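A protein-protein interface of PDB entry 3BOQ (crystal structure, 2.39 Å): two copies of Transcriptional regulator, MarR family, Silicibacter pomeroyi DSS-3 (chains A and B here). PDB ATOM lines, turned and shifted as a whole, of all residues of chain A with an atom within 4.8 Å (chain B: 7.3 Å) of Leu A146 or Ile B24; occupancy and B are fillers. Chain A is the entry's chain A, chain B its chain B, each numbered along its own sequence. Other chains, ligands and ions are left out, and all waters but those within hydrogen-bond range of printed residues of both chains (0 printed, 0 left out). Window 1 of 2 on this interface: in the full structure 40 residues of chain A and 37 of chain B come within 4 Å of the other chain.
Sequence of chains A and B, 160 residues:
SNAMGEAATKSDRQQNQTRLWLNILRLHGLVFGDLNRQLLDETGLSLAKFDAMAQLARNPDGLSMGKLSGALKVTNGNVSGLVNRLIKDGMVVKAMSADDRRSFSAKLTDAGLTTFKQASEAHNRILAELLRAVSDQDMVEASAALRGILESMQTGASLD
The side-chain hydroxyl (OG) of Ser A143 lies within hydrogen-bond range of the side-chain amide nitrogen (ND2) of Asn B23 (2.9 Å).
O of Arg B19 is in hydrogen-bond range of ND2 of Asn B23 (3.4 Å).
The side-chain hydroxyl of Ser A143 is in hydrogen-bond range of the guanidinium group of Arg A147, at 2.7 Å.
OD1 of Asn B23 is in hydrogen-bond range of NH1 of Arg B26 (3.3 Å).
Among the printed residues, merely in contact across the chains: Ile A24 with Leu B27, Ile A24 with His B28, Ile A24 with Leu B146, Leu A27 with Ile B24, Leu A27 with Leu B146, Leu A27 with Ile B149, His A28 with Leu B25, His A28 with His B28, Ala A142 with Leu B20, Ala A145 with Asp B138, Ala A145 with Glu B141, Ala A145 with Ala B142, Leu A146 with Ile B24, Leu A146 with Leu B27, Arg A147 with Asn B23, Gly A148 with Asp B138, Ile A149 with Leu B27, Ile A149 with Asp B138, Ile A149 with Ala B142, Leu A150 with Asn B23, Leu A150 with Arg B26, Leu A150 with Leu B27 and Leu A150 with Leu B30.
Of the printed residues of chain B, Leu A146 touches Ile B24 and Leu B27.
Of the printed residues of chain A, Ile B24 touches Leu A27 (3.4 Å) and Leu A146 (3.9 Å).
Of the printed residues of chain A, Arg B26 touches Leu A150 (3.9 Å).
Printed residues of chain B within 4 Å of Leu A150: Asn B23, Arg B26, Leu B27 and Leu B30.
Printed residues of chain A within 4 Å of Ala B142: Ala A145 and Ile A149.
Printed residues of chain A within 4 Å of Glu B141: Ala A145 (3.98 Å).
The nearest printed residue of chain B that does not touch Leu A146 is Asn B23 (4.02 Å).
The nearest printed residue of chain A that does not touch Glu B141 is Ala A142 (5.1 Å).
Along chain B the printed residues that touch a printed residue of chain A span positions 20 to 149.
Of the 12 printed residues of chain A, 11 touch a printed residue of chain B.
Hydrophobic or aromatic side chains of chain A that line the printed part of chain B: Ile A24, Leu A27, His A28, Ala A142, Ala A145, Leu A146, Ile A149 and Leu A150.
Among the printed residues, 24 pairs touch across the chains.
Among the printed residues, no Asp or Glu carboxylate lies within 4 Å of a Lys or Arg side-chain nitrogen of the other chain.
Ile A24 touches His B28, but with the chains exchanged His A28 does not touch Ile B24 (4.2 Å).
Leu A27 touches Leu B146, and with the chains exchanged Leu A146 touches Leu B27.
His A28 touches its own counterpart, His B28.
Ile A149 touches Ala B142, but with the chains exchanged Ala A142 does not touch Ile B149 (4.03 Å).
Positions printed for both chains: 24, 27, 28, 142, 143, 146 and 149.
Of the 24 pairs that touch across the chains among the printed residues, 9 have their exchanged pair printed and touching as well.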
ATOM      1  N   ILE A  24      24.064  34.582  25.827  1.00  0.00           N
ATOM      2  CA  ILE A  24      22.715  34.044  25.746  1.00  0.00           C
ATOM      3  C   ILE A  24      22.073  34.518  24.467  1.00  0.00           C
ATOM      4  O   ILE A  24      21.579  33.712  23.703  1.00  0.00           O
ATOM      5  CB  ILE A  24      21.837  34.501  26.923  1.00  0.00           C
ATOM      6  CG1 ILE A  24      22.350  33.951  28.269  1.00  0.00           C
ATOM      7  CG2 ILE A  24      20.371  34.025  26.748  1.00  0.00           C
ATOM      8  CD1 ILE A  24      22.005  32.437  28.391  1.00  0.00           C
ATOM      9  N   LEU A  27      23.806  32.730  21.305  1.00  0.00           N
ATOM     10  CA  LEU A  27      23.430  31.329  21.116  1.00  0.00           C
ATOM     11  C   LEU A  27      21.929  31.155  20.765  1.00  0.00           C
ATOM     12  O   LEU A  27      21.578  30.356  19.908  1.00  0.00           O
ATOM     13  CB  LEU A  27      23.803  30.514  22.347  1.00  0.00           C
ATOM     14  CG  LEU A  27      23.497  29.008  22.334  1.00  0.00           C
ATOM     15  CD1 LEU A  27      24.072  28.299  21.127  1.00  0.00           C
ATOM     16  CD2 LEU A  27      24.084  28.410  23.577  1.00  0.00           C
ATOM     17  N   HIS A  28      21.062  31.919  21.421  1.00  0.00           N
ATOM     18  CA  HIS A  28      19.629  31.950  21.079  1.00  0.00           C
ATOM     19  C   HIS A  28      19.432  32.411  19.618  1.00  0.00           C
ATOM     20  O   HIS A  28      18.642  31.836  18.865  1.00  0.00           O
ATOM     21  CB  HIS A  28      18.884  32.861  22.080  1.00  0.00           C
ATOM     22  CG  HIS A  28      17.419  33.010  21.815  1.00  0.00           C
ATOM     23  ND1 HIS A  28      16.916  33.958  20.948  1.00  0.00           N
ATOM     24  CD2 HIS A  28      16.343  32.363  22.331  1.00  0.00           C
ATOM     25  CE1 HIS A  28      15.597  33.874  20.921  1.00  0.00           C
ATOM     26  NE2 HIS A  28      15.225  32.925  21.762  1.00  0.00           N
ATOM     27  N   ALA A 142      27.054  24.174  30.809  1.00  0.00           N
ATOM     28  CA  ALA A 142      26.150  25.321  30.565  1.00  0.00           C
ATOM     29  C   ALA A 142      24.824  25.105  31.289  1.00  0.00           C
ATOM     30  O   ALA A 142      24.310  25.979  31.943  1.00  0.00           O
ATOM     31  CB  ALA A 142      25.872  25.505  29.065  1.00  0.00           C
ATOM     32  N   SER A 143      24.266  23.925  31.152  1.00  0.00           N
ATOM     33  CA  SER A 143      22.935  23.708  31.588  1.00  0.00           C
ATOM     34  C   SER A 143      22.926  23.684  33.127  1.00  0.00           C
ATOM     35  O   SER A 143      22.002  24.183  33.768  1.00  0.00           O
ATOM     36  CB  SER A 143      22.477  22.389  30.960  1.00  0.00           C
ATOM     37  OG  SER A 143      21.222  22.020  31.419  1.00  0.00           O
ATOM     38  N   ALA A 144      23.983  23.139  33.724  1.00  0.00           N
ATOM     39  CA  ALA A 144      24.081  23.082  35.172  1.00  0.00           C
ATOM     40  C   ALA A 144      24.228  24.512  35.734  1.00  0.00           C
ATOM     41  O   ALA A 144      23.615  24.856  36.753  1.00  0.00           O
ATOM     42  CB  ALA A 144      25.257  22.182  35.605  1.00  0.00           C
ATOM     43  N   ALA A 145      25.035  25.334  35.066  1.00  0.00           N
ATOM     44  CA  ALA A 145      25.228  26.710  35.500  1.00  0.00           C
ATOM     45  C   ALA A 145      23.944  27.478  35.259  1.00  0.00           C
ATOM     46  O   ALA A 145      23.588  28.317  36.057  1.00  0.00           O
ATOM     47  CB  ALA A 145      26.400  27.377  34.767  1.00  0.00           C
ATOM     48  N   LEU A 146      23.247  27.200  34.153  1.00  0.00           N
ATOM     49  CA  LEU A 146      22.023  27.949  33.838  1.00  0.00           C
ATOM     50  C   LEU A 146      20.889  27.641  34.795  1.00  0.00           C
ATOM     51  O   LEU A 146      20.159  28.546  35.138  1.00  0.00           O
ATOM     52  CB  LEU A 146      21.565  27.755  32.398  1.00  0.00           C
ATOM     53  CG  LEU A 146      22.455  28.348  31.312  1.00  0.00           C
ATOM     54  CD1 LEU A 146      21.939  27.909  29.933  1.00  0.00           C
ATOM     55  CD2 LEU A 146      22.551  29.850  31.405  1.00  0.00           C
ATOM     56  N   ARG A 147      20.744  26.382  35.209  1.00  0.00           N
ATOM     57  CA  ARG A 147      19.841  26.002  36.306  1.00  0.00           C
ATOM     58  C   ARG A 147      20.184  26.685  37.650  1.00  0.00           C
ATOM     59  O   ARG A 147      19.288  27.120  38.353  1.00  0.00           O
ATOM     60  CB  ARG A 147      19.762  24.466  36.469  1.00  0.00           C
ATOM     61  CG  ARG A 147      19.131  23.770  35.276  1.00  0.00           C
ATOM     62  CD  ARG A 147      18.809  22.240  35.487  1.00  0.00           C
ATOM     63  NE  ARG A 147      19.955  21.431  35.957  1.00  0.00           N
ATOM     64  CZ  ARG A 147      20.856  20.806  35.182  1.00  0.00           C
ATOM     65  NH1 ARG A 147      20.793  20.854  33.851  1.00  0.00           N
ATOM     66  NH2 ARG A 147      21.838  20.120  35.757  1.00  0.00           N
ATOM     67  N   GLY A 148      21.474  26.794  37.993  1.00  0.00           N
ATOM     68  CA  GLY A 148      21.910  27.531  39.182  1.00  0.00           C
ATOM     69  C   GLY A 148      21.364  28.943  39.164  1.00  0.00           C
ATOM     70  O   GLY A 148      20.774  29.415  40.132  1.00  0.00           O
ATOM     71  N   ILE A 149      21.536  29.600  38.023  1.00  0.00           N
ATOM     72  CA  ILE A 149      21.158  31.007  37.784  1.00  0.00           C
ATOM     73  C   ILE A 149      19.651  31.152  37.916  1.00  0.00           C
ATOM     74  O   ILE A 149      19.154  32.049  38.573  1.00  0.00           O
ATOM     75  CB  ILE A 149      21.590  31.442  36.357  1.00  0.00           C
ATOM     76  CG1 ILE A 149      23.125  31.427  36.271  1.00  0.00           C
ATOM     77  CG2 ILE A 149      21.002  32.827  35.979  1.00  0.00           C
ATOM     78  CD1 ILE A 149      23.747  31.744  34.887  1.00  0.00           C
ATOM     79  N   LEU A 150      18.927  30.241  37.287  1.00  0.00           N
ATOM     80  CA  LEU A 150      17.495  30.318  37.230  1.00  0.00           C
ATOM     81  C   LEU A 150      16.866  30.096  38.592  1.00  0.00           C
ATOM     82  O   LEU A 150      15.871  30.737  38.903  1.00  0.00           O
ATOM     83  CB  LEU A 150      16.949  29.302  36.219  1.00  0.00           C
ATOM     84  CG  LEU A 150      17.007  29.697  34.744  1.00  0.00           C
ATOM     85  CD1 LEU A 150      16.965  28.454  33.839  1.00  0.00           C
ATOM     86  CD2 LEU A 150      15.876  30.674  34.425  1.00  0.00           C
ATOM     87  N   GLN B  17      20.696  18.010  25.039  1.00  0.00           N
ATOM     88  CA  GLN B  17      20.356  19.040  24.065  1.00  0.00           C
ATOM     89  C   GLN B  17      18.979  19.666  24.355  1.00  0.00           C
ATOM     90  O   GLN B  17      18.857  20.886  24.442  1.00  0.00           O
ATOM     91  CB  GLN B  17      20.428  18.447  22.656  1.00  0.00           C
ATOM     92  CG  GLN B  17      21.900  18.315  22.160  1.00  0.00           C
ATOM     93  CD  GLN B  17      22.063  17.564  20.855  1.00  0.00           C
ATOM     94  OE1 GLN B  17      21.149  16.918  20.389  1.00  0.00           O
ATOM     95  NE2 GLN B  17      23.243  17.658  20.254  1.00  0.00           N
ATOM     96  N   THR B  18      17.948  18.831  24.499  1.00  0.00           N
ATOM     97  CA  THR B  18      16.638  19.300  24.967  1.00  0.00           C
ATOM     98  C   THR B  18      16.768  20.197  26.200  1.00  0.00           C
ATOM     99  O   THR B  18      16.313  21.341  26.169  1.00  0.00           O
ATOM    100  CB  THR B  18      15.645  18.129  25.181  1.00  0.00           C
ATOM    101  OG1 THR B  18      15.008  17.886  23.932  1.00  0.00           O
ATOM    102  CG2 THR B  18      14.517  18.464  26.216  1.00  0.00           C
ATOM    103  N   ARG B  19      17.411  19.698  27.257  1.00  0.00           N
ATOM    104  CA  ARG B  19      17.557  20.449  28.500  1.00  0.00           C
ATOM    105  C   ARG B  19      18.231  21.775  28.282  1.00  0.00           C
ATOM    106  O   ARG B  19      17.750  22.771  28.777  1.00  0.00           O
ATOM    107  CB  ARG B  19      18.343  19.686  29.556  1.00  0.00           C
ATOM    108  CG  ARG B  19      17.481  18.917  30.502  1.00  0.00           C
ATOM    109  CD  ARG B  19      18.285  18.357  31.667  1.00  0.00           C
ATOM    110  NE  ARG B  19      17.809  17.007  31.992  1.00  0.00           N
ATOM    111  CZ  ARG B  19      18.354  15.878  31.534  1.00  0.00           C
ATOM    112  NH1 ARG B  19      19.432  15.910  30.744  1.00  0.00           N
ATOM    113  NH2 ARG B  19      17.831  14.709  31.892  1.00  0.00           N
ATOM    114  N   LEU B  20      19.343  21.783  27.561  1.00  0.00           N
ATOM    115  CA  LEU B  20      20.140  22.984  27.361  1.00  0.00           C
ATOM    116  C   LEU B  20      19.324  24.097  26.726  1.00  0.00           C
ATOM    117  O   LEU B  20      19.285  25.200  27.230  1.00  0.00           O
ATOM    118  CB  LEU B  20      21.394  22.680  26.493  1.00  0.00           C
ATOM    119  CG  LEU B  20      22.090  23.946  25.946  1.00  0.00           C
ATOM    120  CD1 LEU B  20      22.785  24.687  27.091  1.00  0.00           C
ATOM    121  CD2 LEU B  20      23.049  23.672  24.793  1.00  0.00           C
ATOM    122  N   TRP B  21      18.650  23.774  25.630  1.00  0.00           N
ATOM    123  CA  TRP B  21      17.879  24.715  24.843  1.00  0.00           C
ATOM    124  C   TRP B  21      16.681  25.291  25.609  1.00  0.00           C
ATOM    125  O   TRP B  21      16.427  26.503  25.589  1.00  0.00           O
ATOM    126  CB  TRP B  21      17.426  23.999  23.569  1.00  0.00           C
ATOM    127  CG  TRP B  21      16.536  24.818  22.658  1.00  0.00           C
ATOM    128  CD1 TRP B  21      15.334  24.448  22.152  1.00  0.00           C
ATOM    129  CD2 TRP B  21      16.801  26.143  22.160  1.00  0.00           C
ATOM    130  NE1 TRP B  21      14.828  25.444  21.361  1.00  0.00           N
ATOM    131  CE2 TRP B  21      15.710  26.496  21.336  1.00  0.00           C
ATOM    132  CE3 TRP B  21      17.865  27.071  22.335  1.00  0.00           C
ATOM    133  CZ2 TRP B  21      15.623  27.741  20.695  1.00  0.00           C
ATOM    134  CZ3 TRP B  21      17.794  28.308  21.669  1.00  0.00           C
ATOM    135  CH2 TRP B  21      16.673  28.630  20.871  1.00  0.00           C
ATOM    136  N   LEU B  22      15.933  24.412  26.268  1.00  0.00           N
ATOM    137  CA  LEU B  22      14.909  24.846  27.233  1.00  0.00           C
ATOM    138  C   LEU B  22      15.478  25.816  28.300  1.00  0.00           C
ATOM    139  O   LEU B  22      14.836  26.823  28.594  1.00  0.00           O
ATOM    140  CB  LEU B  22      14.207  23.631  27.863  1.00  0.00           C
ATOM    141  CG  LEU B  22      12.833  23.191  27.301  1.00  0.00           C
ATOM    142  CD1 LEU B  22      12.698  23.330  25.784  1.00  0.00           C
ATOM    143  CD2 LEU B  22      12.454  21.778  27.730  1.00  0.00           C
ATOM    144  N   ASN B  23      16.662  25.535  28.861  1.00  0.00           N
ATOM    145  CA  ASN B  23      17.313  26.462  29.820  1.00  0.00           C
ATOM    146  C   ASN B  23      17.690  27.821  29.237  1.00  0.00           C
ATOM    147  O   ASN B  23      17.519  28.839  29.880  1.00  0.00           O
ATOM    148  CB  ASN B  23      18.540  25.833  30.463  1.00  0.00           C
ATOM    149  CG  ASN B  23      18.162  24.837  31.525  1.00  0.00           C
ATOM    150  OD1 ASN B  23      17.093  24.949  32.121  1.00  0.00           O
ATOM    151  ND2 ASN B  23      19.024  23.855  31.774  1.00  0.00           N
ATOM    152  N   ILE B  24      18.199  27.826  28.014  1.00  0.00           N
ATOM    153  CA  ILE B  24      18.502  29.041  27.351  1.00  0.00           C
ATOM    154  C   ILE B  24      17.245  29.848  27.122  1.00  0.00           C
ATOM    155  O   ILE B  24      17.225  31.037  27.367  1.00  0.00           O
ATOM    156  CB  ILE B  24      19.170  28.780  26.018  1.00  0.00           C
ATOM    157  CG1 ILE B  24      20.595  28.285  26.245  1.00  0.00           C
ATOM    158  CG2 ILE B  24      19.138  30.028  25.179  1.00  0.00           C
ATOM    159  CD1 ILE B  24      21.167  27.589  25.044  1.00  0.00           C
ATOM    160  N   LEU B  25      16.208  29.194  26.641  1.00  0.00           N
ATOM    161  CA  LEU B  25      14.918  29.829  26.421  1.00  0.00           C
ATOM    162  C   LEU B  25      14.296  30.406  27.697  1.00  0.00           C
ATOM    163  O   LEU B  25      13.762  31.520  27.663  1.00  0.00           O
ATOM    164  CB  LEU B  25      13.945  28.856  25.739  1.00  0.00           C
ATOM    165  CG  LEU B  25      14.089  28.628  24.227  1.00  0.00           C
ATOM    166  CD1 LEU B  25      13.043  27.580  23.756  1.00  0.00           C
ATOM    167  CD2 LEU B  25      13.901  29.920  23.393  1.00  0.00           C
ATOM    168  N   ARG B  26      14.365  29.661  28.805  1.00  0.00           N
ATOM    169  CA  ARG B  26      13.939  30.133  30.126  1.00  0.00           C
ATOM    170  C   ARG B  26      14.710  31.391  30.539  1.00  0.00           C
ATOM    171  O   ARG B  26      14.103  32.379  30.921  1.00  0.00           O
ATOM    172  CB  ARG B  26      14.144  29.056  31.200  1.00  0.00           C
ATOM    173  CG  ARG B  26      13.078  28.026  31.300  1.00  0.00           C
ATOM    174  CD  ARG B  26      13.615  26.704  31.872  1.00  0.00           C
ATOM    175  NE  ARG B  26      12.589  25.648  31.934  1.00  0.00           N
ATOM    176  CZ  ARG B  26      12.826  24.338  31.771  1.00  0.00           C
ATOM    177  NH1 ARG B  26      14.058  23.893  31.531  1.00  0.00           N
ATOM    178  NH2 ARG B  26      11.826  23.463  31.834  1.00  0.00           N
ATOM    179  N   LEU B  27      16.035  31.367  30.490  1.00  0.00           N
ATOM    180  CA  LEU B  27      16.787  32.513  30.984  1.00  0.00           C
ATOM    181  C   LEU B  27      16.544  33.666  29.999  1.00  0.00           C
ATOM    182  O   LEU B  27      16.199  34.778  30.399  1.00  0.00           O
ATOM    183  CB  LEU B  27      18.275  32.193  31.156  1.00  0.00           C
ATOM    184  CG  LEU B  27      19.146  33.260  31.824  1.00  0.00           C
ATOM    185  CD1 LEU B  27      18.623  33.592  33.191  1.00  0.00           C
ATOM    186  CD2 LEU B  27      20.595  32.804  31.940  1.00  0.00           C
ATOM    187  N   HIS B  28      16.668  33.385  28.708  1.00  0.00           N
ATOM    188  CA  HIS B  28      16.452  34.418  27.719  1.00  0.00           C
ATOM    189  C   HIS B  28      15.111  35.145  27.917  1.00  0.00           C
ATOM    190  O   HIS B  28      15.089  36.374  27.963  1.00  0.00           O
ATOM    191  CB  HIS B  28      16.527  33.874  26.307  1.00  0.00           C
ATOM    192  CG  HIS B  28      16.183  34.893  25.276  1.00  0.00           C
ATOM    193  ND1 HIS B  28      14.887  35.143  24.889  1.00  0.00           N
ATOM    194  CD2 HIS B  28      16.958  35.750  24.575  1.00  0.00           C
ATOM    195  CE1 HIS B  28      14.875  36.080  23.960  1.00  0.00           C
ATOM    196  NE2 HIS B  28      16.121  36.469  23.754  1.00  0.00           N
ATOM    197  N   GLY B  29      14.016  34.387  28.045  1.00  0.00           N
ATOM    198  CA  GLY B  29      12.685  34.946  28.297  1.00  0.00           C
ATOM    199  C   GLY B  29      12.501  35.714  29.601  1.00  0.00           C
ATOM    200  O   GLY B  29      11.814  36.759  29.614  1.00  0.00           O
ATOM    201  N   LEU B  30      13.070  35.189  30.695  1.00  0.00           N
ATOM    202  CA  LEU B  30      12.983  35.795  32.017  1.00  0.00           C
ATOM    203  C   LEU B  30      13.716  37.135  32.049  1.00  0.00           C
ATOM    204  O   LEU B  30      13.322  38.051  32.759  1.00  0.00           O
ATOM    205  CB  LEU B  30      13.638  34.894  33.066  1.00  0.00           C
ATOM    206  CG  LEU B  30      12.880  34.199  34.191  1.00  0.00           C
ATOM    207  CD1 LEU B  30      13.870  33.788  35.273  1.00  0.00           C
ATOM    208  CD2 LEU B  30      11.794  35.082  34.792  1.00  0.00           C
ATOM    209  N   ASP B 138      28.389  31.027  39.032  1.00  0.00           N
ATOM    210  CA  ASP B 138      27.407  30.501  38.070  1.00  0.00           C
ATOM    211  C   ASP B 138      27.452  31.252  36.742  1.00  0.00           C
ATOM    212  O   ASP B 138      27.337  30.614  35.691  1.00  0.00           O
ATOM    213  CB  ASP B 138      25.998  30.558  38.627  1.00  0.00           C
ATOM    214  CG  ASP B 138      25.655  29.358  39.466  1.00  0.00           C
ATOM    215  OD1 ASP B 138      26.415  28.362  39.482  1.00  0.00           O
ATOM    216  OD2 ASP B 138      24.600  29.392  40.121  1.00  0.00           O
ATOM    217  N   GLU B 141      30.771  30.441  34.926  1.00  0.00           N
ATOM    218  CA  GLU B 141      30.712  29.066  34.401  1.00  0.00           C
ATOM    219  C   GLU B 141      29.736  28.895  33.224  1.00  0.00           C
ATOM    220  O   GLU B 141      30.070  28.187  32.266  1.00  0.00           O
ATOM    221  CB  GLU B 141      30.466  28.045  35.519  1.00  0.00           C
ATOM    222  CG  GLU B 141      31.690  27.939  36.448  1.00  0.00           C
ATOM    223  CD  GLU B 141      31.475  27.082  37.681  1.00  0.00           C
ATOM    224  OE1 GLU B 141      30.315  26.794  38.044  1.00  0.00           O
ATOM    225  OE2 GLU B 141      32.480  26.696  38.311  1.00  0.00           O
ATOM    226  N   ALA B 142      28.547  29.530  33.300  1.00  0.00           N
ATOM    227  CA  ALA B 142      27.595  29.577  32.187  1.00  0.00           C
ATOM    228  C   ALA B 142      28.302  30.221  30.996  1.00  0.00           C
ATOM    229  O   ALA B 142      28.355  29.664  29.903  1.00  0.00           O
ATOM    230  CB  ALA B 142      26.373  30.399  32.561  1.00  0.00           C
ATOM    231  N   SER B 143      28.900  31.378  31.222  1.00  0.00           N
ATOM    232  CA  SER B 143      29.540  32.046  30.146  1.00  0.00           C
ATOM    233  C   SER B 143      30.685  31.243  29.499  1.00  0.00           C
ATOM    234  O   SER B 143      30.770  31.196  28.275  1.00  0.00           O
ATOM    235  CB  SER B 143      30.047  33.389  30.612  1.00  0.00           C
ATOM    236  OG  SER B 143      29.650  34.338  29.683  1.00  0.00           O
ATOM    237  N   LEU B 146      28.999  28.529  27.425  1.00  0.00           N
ATOM    238  CA  LEU B 146      28.305  29.023  26.223  1.00  0.00           C
ATOM    239  C   LEU B 146      29.278  29.486  25.124  1.00  0.00           C
ATOM    240  O   LEU B 146      29.031  29.252  23.938  1.00  0.00           O
ATOM    241  CB  LEU B 146      27.366  30.140  26.582  1.00  0.00           C
ATOM    242  CG  LEU B 146      26.204  29.838  27.517  1.00  0.00           C
ATOM    243  CD1 LEU B 146      25.522  31.172  27.867  1.00  0.00           C
ATOM    244  CD2 LEU B 146      25.191  28.830  26.927  1.00  0.00           C
ATOM    245  N   ILE B 149      30.431  26.360  23.429  1.00  0.00           N
ATOM    246  CA  ILE B 149      29.359  25.970  22.500  1.00  0.00           C
ATOM    247  C   ILE B 149      29.390  26.791  21.206  1.00  0.00           C
ATOM    248  O   ILE B 149      29.415  26.231  20.116  1.00  0.00           O
ATOM    249  CB  ILE B 149      27.977  26.074  23.175  1.00  0.00           C
ATOM    250  CG1 ILE B 149      27.868  25.031  24.298  1.00  0.00           C
ATOM    251  CG2 ILE B 149      26.855  25.826  22.173  1.00  0.00           C
ATOM    252  CD1 ILE B 149      26.612  25.111  25.120  1.00  0.00           C
